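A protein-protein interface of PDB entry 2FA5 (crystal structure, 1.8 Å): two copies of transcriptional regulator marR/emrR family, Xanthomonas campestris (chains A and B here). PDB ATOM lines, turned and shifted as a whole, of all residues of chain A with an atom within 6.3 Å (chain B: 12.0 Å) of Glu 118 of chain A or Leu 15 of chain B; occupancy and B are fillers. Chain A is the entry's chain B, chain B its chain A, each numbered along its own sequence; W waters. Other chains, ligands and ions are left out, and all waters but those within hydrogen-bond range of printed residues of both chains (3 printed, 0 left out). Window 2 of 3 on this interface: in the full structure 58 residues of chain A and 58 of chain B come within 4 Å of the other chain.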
ATOM      1  N   TRP A  52      38.975   5.343  21.220  1.00  0.00           N
ATOM      2  CA  TRP A  52      37.731   6.090  21.344  1.00  0.00           C
ATOM      3  C   TRP A  52      36.898   5.870  20.080  1.00  0.00           C
ATOM      4  O   TRP A  52      35.689   5.684  20.156  1.00  0.00           O
ATOM      5  CB  TRP A  52      38.014   7.584  21.540  1.00  0.00           C
ATOM      6  CG  TRP A  52      36.795   8.451  21.395  1.00  0.00           C
ATOM      7  CD1 TRP A  52      36.555   9.377  20.413  1.00  0.00           C
ATOM      8  CD2 TRP A  52      35.643   8.460  22.243  1.00  0.00           C
ATOM      9  NE1 TRP A  52      35.321   9.959  20.601  1.00  0.00           N
ATOM     10  CE2 TRP A  52      34.742   9.414  21.718  1.00  0.00           C
ATOM     11  CE3 TRP A  52      35.282   7.750  23.398  1.00  0.00           C
ATOM     12  CZ2 TRP A  52      33.502   9.679  22.309  1.00  0.00           C
ATOM     13  CZ3 TRP A  52      34.052   8.012  23.985  1.00  0.00           C
ATOM     14  CH2 TRP A  52      33.175   8.971  23.437  1.00  0.00           C
ATOM     15  N   ALA A  59      28.949   1.715  19.622  1.00  0.00           N
ATOM     16  CA  ALA A  59      27.736   2.258  20.227  1.00  0.00           C
ATOM     17  C   ALA A  59      26.659   2.386  19.151  1.00  0.00           C
ATOM     18  O   ALA A  59      25.489   2.102  19.391  1.00  0.00           O
ATOM     19  CB  ALA A  59      28.015   3.620  20.846  1.00  0.00           C
ATOM     20  N   GLY A 113      32.374   0.140  29.272  1.00  0.00           N
ATOM     21  CA  GLY A 113      32.681   0.956  28.112  1.00  0.00           C
ATOM     22  C   GLY A 113      31.562   1.944  27.828  1.00  0.00           C
ATOM     23  O   GLY A 113      31.817   3.070  27.391  1.00  0.00           O
ATOM     24  N   ARG A 114      30.323   1.532  28.083  1.00  0.00           N
ATOM     25  CA  ARG A 114      29.171   2.399  27.836  1.00  0.00           C
ATOM     26  C   ARG A 114      29.162   3.565  28.816  1.00  0.00           C
ATOM     27  O   ARG A 114      28.754   4.669  28.469  1.00  0.00           O
ATOM     28  CB  ARG A 114      27.861   1.608  27.941  1.00  0.00           C
ATOM     29  CG  ARG A 114      26.627   2.424  27.536  1.00  0.00           C
ATOM     30  CD  ARG A 114      25.391   1.553  27.369  1.00  0.00           C
ATOM     31  NE  ARG A 114      25.531   0.574  26.292  1.00  0.00           N
ATOM     32  CZ  ARG A 114      25.623   0.874  24.998  1.00  0.00           C
ATOM     33  NH1 ARG A 114      25.591   2.140  24.595  1.00  0.00           N
ATOM     34  NH2 ARG A 114      25.749  -0.097  24.101  1.00  0.00           N
ATOM     35  N   GLN A 115      29.617   3.317  30.042  1.00  0.00           N
ATOM     36  CA  GLN A 115      29.688   4.368  31.056  1.00  0.00           C
ATOM     37  C   GLN A 115      30.694   5.420  30.587  1.00  0.00           C
ATOM     38  O   GLN A 115      30.474   6.625  30.735  1.00  0.00           O
ATOM     39  CB  GLN A 115      30.120   3.771  32.399  1.00  0.00           C
ATOM     40  CG  GLN A 115      30.534   4.787  33.462  1.00  0.00           C
ATOM     41  CD  GLN A 115      29.488   5.848  33.714  1.00  0.00           C
ATOM     42  OE1 GLN A 115      28.286   5.573  33.697  1.00  0.00           O
ATOM     43  NE2 GLN A 115      29.941   7.073  33.970  1.00  0.00           N
ATOM     44  N   VAL A 116      31.802   4.960  30.009  1.00  0.00           N
ATOM     45  CA  VAL A 116      32.815   5.876  29.499  1.00  0.00           C
ATOM     46  C   VAL A 116      32.205   6.671  28.343  1.00  0.00           C
ATOM     47  O   VAL A 116      32.322   7.895  28.284  1.00  0.00           O
ATOM     48  CB  VAL A 116      34.056   5.105  28.991  1.00  0.00           C
ATOM     49  CG1 VAL A 116      35.031   6.063  28.310  1.00  0.00           C
ATOM     50  CG2 VAL A 116      34.741   4.397  30.163  1.00  0.00           C
ATOM     51  N   TYR A 117      31.547   5.959  27.433  1.00  0.00           N
ATOM     52  CA  TYR A 117      30.905   6.565  26.267  1.00  0.00           C
ATOM     53  C   TYR A 117      29.913   7.651  26.662  1.00  0.00           C
ATOM     54  O   TYR A 117      29.940   8.755  26.119  1.00  0.00           O
ATOM     55  CB  TYR A 117      30.172   5.488  25.464  1.00  0.00           C
ATOM     56  CG  TYR A 117      29.388   5.997  24.267  1.00  0.00           C
ATOM     57  CD1 TYR A 117      30.038   6.529  23.152  1.00  0.00           C
ATOM     58  CD2 TYR A 117      27.994   5.902  24.235  1.00  0.00           C
ATOM     59  CE1 TYR A 117      29.316   6.948  22.026  1.00  0.00           C
ATOM     60  CE2 TYR A 117      27.263   6.319  23.123  1.00  0.00           C
ATOM     61  CZ  TYR A 117      27.931   6.838  22.021  1.00  0.00           C
ATOM     62  OH  TYR A 117      27.206   7.219  20.917  1.00  0.00           O
ATOM     63  N   GLU A 118      29.034   7.336  27.608  1.00  0.00           N
ATOM     64  CA  GLU A 118      28.024   8.301  28.036  1.00  0.00           C
ATOM     65  C   GLU A 118      28.620   9.499  28.777  1.00  0.00           C
ATOM     66  O   GLU A 118      28.022  10.575  28.813  1.00  0.00           O
ATOM     67  CB  GLU A 118      26.957   7.586  28.882  1.00  0.00           C
ATOM     68  CG  GLU A 118      26.350   6.396  28.132  1.00  0.00           C
ATOM     69  CD  GLU A 118      25.181   5.747  28.849  1.00  0.00           C
ATOM     70  OE1 GLU A 118      25.246   5.597  30.089  1.00  0.00           O
ATOM     71  OE2 GLU A 118      24.205   5.369  28.163  1.00  0.00           O
ATOM     72  N   THR A 119      29.813   9.327  29.335  1.00  0.00           N
ATOM     73  CA  THR A 119      30.465  10.415  30.054  1.00  0.00           C
ATOM     74  C   THR A 119      31.224  11.331  29.097  1.00  0.00           C
ATOM     75  O   THR A 119      31.238  12.551  29.266  1.00  0.00           O
ATOM     76  CB  THR A 119      31.474   9.881  31.098  1.00  0.00           C
ATOM     77  OG1 THR A 119      30.789   9.070  32.061  1.00  0.00           O
ATOM     78  CG2 THR A 119      32.163  11.041  31.812  1.00  0.00           C
ATOM     79  N   VAL A 120      31.832  10.733  28.078  1.00  0.00           N
ATOM     80  CA  VAL A 120      32.644  11.474  27.117  1.00  0.00           C
ATOM     81  C   VAL A 120      31.885  12.074  25.934  1.00  0.00           C
ATOM     82  O   VAL A 120      32.131  13.222  25.549  1.00  0.00           O
ATOM     83  CB  VAL A 120      33.790  10.565  26.587  1.00  0.00           C
ATOM     84  CG1 VAL A 120      34.624  11.298  25.541  1.00  0.00           C
ATOM     85  CG2 VAL A 120      34.681  10.133  27.749  1.00  0.00           C
ATOM     86  N   ALA A 121      30.962  11.303  25.369  1.00  0.00           N
ATOM     87  CA  ALA A 121      30.182  11.736  24.211  1.00  0.00           C
ATOM     88  C   ALA A 121      29.618  13.153  24.315  1.00  0.00           C
ATOM     89  O   ALA A 121      29.784  13.959  23.398  1.00  0.00           O
ATOM     90  CB  ALA A 121      29.053  10.743  23.947  1.00  0.00           C
ATOM     91  N   PRO A 122      28.935  13.477  25.428  1.00  0.00           N
ATOM     92  CA  PRO A 122      28.363  14.819  25.593  1.00  0.00           C
ATOM     93  C   PRO A 122      29.398  15.928  25.415  1.00  0.00           C
ATOM     94  O   PRO A 122      29.144  16.927  24.740  1.00  0.00           O
ATOM     95  CB  PRO A 122      27.799  14.782  27.014  1.00  0.00           C
ATOM     96  CG  PRO A 122      27.404  13.340  27.176  1.00  0.00           C
ATOM     97  CD  PRO A 122      28.594  12.617  26.577  1.00  0.00           C
ATOM     98  N   ASN A 125      30.467  16.235  21.777  1.00  0.00           N
ATOM     99  CA  ASN A 125      29.442  16.921  20.989  1.00  0.00           C
ATOM    100  C   ASN A 125      29.550  18.425  21.205  1.00  0.00           C
ATOM    101  O   ASN A 125      29.412  19.216  20.268  1.00  0.00           O
ATOM    102  CB  ASN A 125      28.040  16.468  21.403  1.00  0.00           C
ATOM    103  CG  ASN A 125      27.544  15.291  20.593  1.00  0.00           C
ATOM    104  OD1 ASN A 125      27.650  15.283  19.364  1.00  0.00           O
ATOM    105  ND2 ASN A 125      26.981  14.297  21.272  1.00  0.00           N
ATOM    106  N   HIS B  12      20.003   1.747  25.328  1.00  0.00           N
ATOM    107  CA  HIS B  12      21.344   2.347  25.077  1.00  0.00           C
ATOM    108  C   HIS B  12      21.253   3.379  23.958  1.00  0.00           C
ATOM    109  O   HIS B  12      21.346   3.040  22.779  1.00  0.00           O
ATOM    110  CB  HIS B  12      22.344   1.260  24.682  1.00  0.00           C
ATOM    111  CG  HIS B  12      22.415   0.119  25.649  1.00  0.00           C
ATOM    112  ND1 HIS B  12      22.516   0.303  27.011  1.00  0.00           N
ATOM    113  CD2 HIS B  12      22.428  -1.220  25.448  1.00  0.00           C
ATOM    114  CE1 HIS B  12      22.589  -0.873  27.608  1.00  0.00           C
ATOM    115  NE2 HIS B  12      22.537  -1.814  26.682  1.00  0.00           N
ATOM    116  N   PRO B  13      21.077   4.659  24.314  1.00  0.00           N
ATOM    117  CA  PRO B  13      20.975   5.718  23.310  1.00  0.00           C
ATOM    118  C   PRO B  13      22.295   6.047  22.619  1.00  0.00           C
ATOM    119  O   PRO B  13      23.371   5.909  23.206  1.00  0.00           O
ATOM    120  CB  PRO B  13      20.453   6.896  24.119  1.00  0.00           C
ATOM    121  CG  PRO B  13      21.169   6.709  25.426  1.00  0.00           C
ATOM    122  CD  PRO B  13      20.982   5.222  25.676  1.00  0.00           C
ATOM    123  N   VAL B  14      22.202   6.472  21.364  1.00  0.00           N
ATOM    124  CA  VAL B  14      23.381   6.866  20.603  1.00  0.00           C
ATOM    125  C   VAL B  14      23.543   8.358  20.880  1.00  0.00           C
ATOM    126  O   VAL B  14      22.667   9.159  20.548  1.00  0.00           O
ATOM    127  CB  VAL B  14      23.182   6.639  19.094  1.00  0.00           C
ATOM    128  CG1 VAL B  14      24.430   7.063  18.334  1.00  0.00           C
ATOM    129  CG2 VAL B  14      22.879   5.182  18.828  1.00  0.00           C
ATOM    130  N   LEU B  15      24.655   8.726  21.506  1.00  0.00           N
ATOM    131  CA  LEU B  15      24.910  10.118  21.850  1.00  0.00           C
ATOM    132  C   LEU B  15      25.734  10.836  20.795  1.00  0.00           C
ATOM    133  O   LEU B  15      25.720  12.065  20.710  1.00  0.00           O
ATOM    134  CB  LEU B  15      25.620  10.194  23.201  1.00  0.00           C
ATOM    135  CG  LEU B  15      24.832   9.611  24.375  1.00  0.00           C
ATOM    136  CD1 LEU B  15      25.673   9.692  25.638  1.00  0.00           C
ATOM    137  CD2 LEU B  15      23.524  10.376  24.543  1.00  0.00           C
ATOM    138  N   LEU B  16      26.456  10.063  19.994  1.00  0.00           N
ATOM    139  CA  LEU B  16      27.282  10.627  18.939  1.00  0.00           C
ATOM    140  C   LEU B  16      26.827  10.034  17.608  1.00  0.00           C
ATOM    141  O   LEU B  16      27.167   8.901  17.276  1.00  0.00           O
ATOM    142  CB  LEU B  16      28.751  10.294  19.204  1.00  0.00           C
ATOM    143  CG  LEU B  16      29.813  11.169  18.539  1.00  0.00           C
ATOM    144  CD1 LEU B  16      29.612  12.624  18.932  1.00  0.00           C
ATOM    145  CD2 LEU B  16      31.194  10.692  18.972  1.00  0.00           C
ATOM    146  N   ASN B  17      26.039  10.805  16.859  1.00  0.00           N
ATOM    147  CA  ASN B  17      25.519  10.358  15.568  1.00  0.00           C
ATOM    148  C   ASN B  17      26.591  10.522  14.497  1.00  0.00           C
ATOM    149  O   ASN B  17      26.532  11.440  13.673  1.00  0.00           O
ATOM    150  CB  ASN B  17      24.275  11.172  15.199  1.00  0.00           C
ATOM    151  CG  ASN B  17      23.490  10.553  14.064  1.00  0.00           C
ATOM    152  OD1 ASN B  17      23.094   9.389  14.134  1.00  0.00           O
ATOM    153  ND2 ASN B  17      23.249  11.328  13.015  1.00  0.00           N
ATOM    154  N   LEU B  18      27.559   9.610  14.514  1.00  0.00           N
ATOM    155  CA  LEU B  18      28.693   9.629  13.595  1.00  0.00           C
ATOM    156  C   LEU B  18      28.411   9.931  12.128  1.00  0.00           C
ATOM    157  O   LEU B  18      29.095  10.749  11.525  1.00  0.00           O
ATOM    158  CB  LEU B  18      29.450   8.299  13.676  1.00  0.00           C
ATOM    159  CG  LEU B  18      30.108   7.930  15.008  1.00  0.00           C
ATOM    160  CD1 LEU B  18      30.808   6.592  14.863  1.00  0.00           C
ATOM    161  CD2 LEU B  18      31.098   9.003  15.422  1.00  0.00           C
ATOM    162  N   GLU B  19      27.423   9.259  11.545  1.00  0.00           N
ATOM    163  CA  GLU B  19      27.123   9.464  10.133  1.00  0.00           C
ATOM    164  C   GLU B  19      26.880  10.919   9.751  1.00  0.00           C
ATOM    165  O   GLU B  19      27.061  11.296   8.593  1.00  0.00           O
ATOM    166  CB  GLU B  19      25.927   8.604   9.712  1.00  0.00           C
ATOM    167  CG  GLU B  19      26.154   7.100   9.853  1.00  0.00           C
ATOM    168  CD  GLU B  19      27.491   6.637   9.284  1.00  0.00           C
ATOM    169  OE1 GLU B  19      27.993   7.254   8.319  1.00  0.00           O
ATOM    170  OE2 GLU B  19      28.033   5.638   9.796  1.00  0.00           O
ATOM    171  N   GLN B  20      26.478  11.740  10.715  1.00  0.00           N
ATOM    172  CA  GLN B  20      26.232  13.150  10.440  1.00  0.00           C
ATOM    173  C   GLN B  20      27.150  14.045  11.268  1.00  0.00           C
ATOM    174  O   GLN B  20      26.940  15.251  11.353  1.00  0.00           O
ATOM    175  CB  GLN B  20      24.769  13.499  10.731  1.00  0.00           C
ATOM    176  CG  GLN B  20      23.766  12.687   9.927  1.00  0.00           C
ATOM    177  CD  GLN B  20      22.350  13.214  10.053  1.00  0.00           C
ATOM    178  OE1 GLN B  20      21.835  13.386  11.158  1.00  0.00           O
ATOM    179  NE2 GLN B  20      21.711  13.469   8.916  1.00  0.00           N
ATOM    180  N   PHE B  21      28.175  13.439  11.863  1.00  0.00           N
ATOM    181  CA  PHE B  21      29.139  14.145  12.707  1.00  0.00           C
ATOM    182  C   PHE B  21      30.317  14.608  11.841  1.00  0.00           C
ATOM    183  O   PHE B  21      31.117  13.792  11.381  1.00  0.00           O
ATOM    184  CB  PHE B  21      29.613  13.186  13.810  1.00  0.00           C
ATOM    185  CG  PHE B  21      30.333  13.854  14.948  1.00  0.00           C
ATOM    186  CD1 PHE B  21      29.709  14.844  15.701  1.00  0.00           C
ATOM    187  CD2 PHE B  21      31.621  13.466  15.292  1.00  0.00           C
ATOM    188  CE1 PHE B  21      30.360  15.433  16.783  1.00  0.00           C
ATOM    189  CE2 PHE B  21      32.282  14.049  16.370  1.00  0.00           C
ATOM    190  CZ  PHE B  21      31.648  15.036  17.119  1.00  0.00           C
ATOM    191  N   LEU B  22      30.422  15.918  11.626  1.00  0.00           N
ATOM    192  CA  LEU B  22      31.479  16.486  10.786  1.00  0.00           C
ATOM    193  C   LEU B  22      32.894  15.933  11.003  1.00  0.00           C
ATOM    194  O   LEU B  22      33.564  15.557  10.041  1.00  0.00           O
ATOM    195  CB  LEU B  22      31.497  18.012  10.932  1.00  0.00           C
ATOM    196  CG  LEU B  22      32.346  18.845   9.963  1.00  0.00           C
ATOM    197  CD1 LEU B  22      33.832  18.700  10.274  1.00  0.00           C
ATOM    198  CD2 LEU B  22      32.033  18.423   8.538  1.00  0.00           C
ATOM    199  N   PRO B  23      33.377  15.895  12.256  1.00  0.00           N
ATOM    200  CA  PRO B  23      34.729  15.370  12.484  1.00  0.00           C
ATOM    201  C   PRO B  23      34.919  13.963  11.917  1.00  0.00           C
ATOM    202  O   PRO B  23      35.985  13.625  11.385  1.00  0.00           O
ATOM    203  CB  PRO B  23      34.860  15.410  14.005  1.00  0.00           C
ATOM    204  CG  PRO B  23      34.040  16.625  14.369  1.00  0.00           C
ATOM    205  CD  PRO B  23      32.805  16.435  13.504  1.00  0.00           C
ATOM    206  N   TYR B  24      33.882  13.144  12.036  1.00  0.00           N
ATOM    207  CA  TYR B  24      33.927  11.777  11.537  1.00  0.00           C
ATOM    208  C   TYR B  24      33.905  11.788  10.013  1.00  0.00           C
ATOM    209  O   TYR B  24      34.716  11.129   9.370  1.00  0.00           O
ATOM    210  CB  TYR B  24      32.730  10.982  12.068  1.00  0.00           C
ATOM    211  CG  TYR B  24      32.723   9.526  11.654  1.00  0.00           C
ATOM    212  CD1 TYR B  24      33.678   8.638  12.146  1.00  0.00           C
ATOM    213  CD2 TYR B  24      31.758   9.034  10.775  1.00  0.00           C
ATOM    214  CE1 TYR B  24      33.671   7.298  11.775  1.00  0.00           C
ATOM    215  CE2 TYR B  24      31.743   7.698  10.397  1.00  0.00           C
ATOM    216  CZ  TYR B  24      32.703   6.836  10.900  1.00  0.00           C
ATOM    217  OH  TYR B  24      32.698   5.510  10.529  1.00  0.00           O
HETATM  218  O   HOH W   1      28.602   6.975  18.654  1.00  0.00           O
HETATM  219  O   HOH W   2      26.085  13.656  17.737  1.00  0.00           O
HETATM  220  O   HOH W   3      24.632   4.514  25.280  1.00  0.00           O
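N of Leu 15 of chain B is in hydrogen-bond range of OH of Tyr 117 of chain A, at 3.0 Å.
The backbone carbonyl oxygen (O) of Leu 15 of chain B sits at hydrogen-bond distance from the side-chain amide nitrogen (ND2) of Asn 125 of chain A (2.6 Å).
A ring nitrogen (ND1) of His 12 of chain B lies within hydrogen-bond range of the guanidinium group (NE) of Arg 114 of chain A (3.1 Å).
N of Leu 16 of chain B is in hydrogen-bond range of OH of Tyr 117 of chain A (3.1 Å).
Tyr 117 of chain A touches Pro 13 of chain B (CE2 to O, 3.9 Å).
Tyr 117 of chain A touches Val 14 of chain B (OH to CG1, 3.8 Å).
CA of Glu 118 of chain A touches CD1 of Leu 15 of chain B (3.6 Å).
Leu 15 of chain B touches Ala 121 of chain A.
OD1 of Asn 125 of chain A touches CD1 of Leu 16 of chain B (3.3 Å).
OD1 of Asn 125 of chain A touches CE1 of Phe 21 of chain B, at 3.7 Å.
Val 116 of chain A touches none of the printed residues of chain B.
Glu 118 of chain A touches one residue of chain B.
Printed residues of chain B within 4 Å of Asn 125 of chain A: Leu 15 (2.6 Å), Leu 16 (3.3 Å) and Phe 21 (3.7 Å).
Of the printed residues of chain A, His 12 of chain B touches Arg 114 (3.1 Å).
Printed residues of chain A within 4 Å of Pro 13 of chain B: Tyr 117 (3.9 Å).
Of the printed residues of chain A, Val 14 of chain B touches Tyr 117 (3.8 Å).
Leu 15 of chain B touches four residues of chain A.
Of the printed residues of chain A, Phe 21 of chain B touches Asn 125 (3.7 Å).
Pro 23 of chain B touches none of the printed residues of chain A.
The nearest residue of chain B that does not touch Glu 118 of chain A is Pro 13 of chain B (4.1 Å).
Of the 13 printed residues of chain A, 5 touch a printed residue of chain B.
Printed residues of chain A that touch a printed residue of chain B: Arg 114, Tyr 117, Glu 118, Ala 121 and Asn 125.
Hydrophobic or aromatic side chains of chain A that line the printed part of chain B: Tyr 117 and Ala 121.
Along chain A the printed residues that touch a printed residue of chain B span positions 114 to 125.
Of the 13 printed residues of chain B, 6 touch a printed residue of chain A.
Among the printed residues, no Asp or Glu carboxylate lies within 4 Å of a Lys or Arg side-chain nitrogen of the other chain.
No position is printed for both chains.
Water W3 lies within hydrogen-bond range of NH1 of Arg 114 of chain A (2.7 Å), O of Pro 13 of chain B (2.8 Å) and OE2 of Glu 118 of chain A (3.0 Å).
Water W1 bridges the side-chain hydroxyl (OH) of Tyr 117 of chain A (2.7 Å) and the backbone carbonyl oxygen (O) of Leu 16 of chain B (2.8 Å).
Water W2 lies within hydrogen-bond range of OD1 of Asn 125 of chain A (2.8 Å), N of Asn 17 of chain B (3.0 Å) and O of Leu 15 of chain B (3.4 Å).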
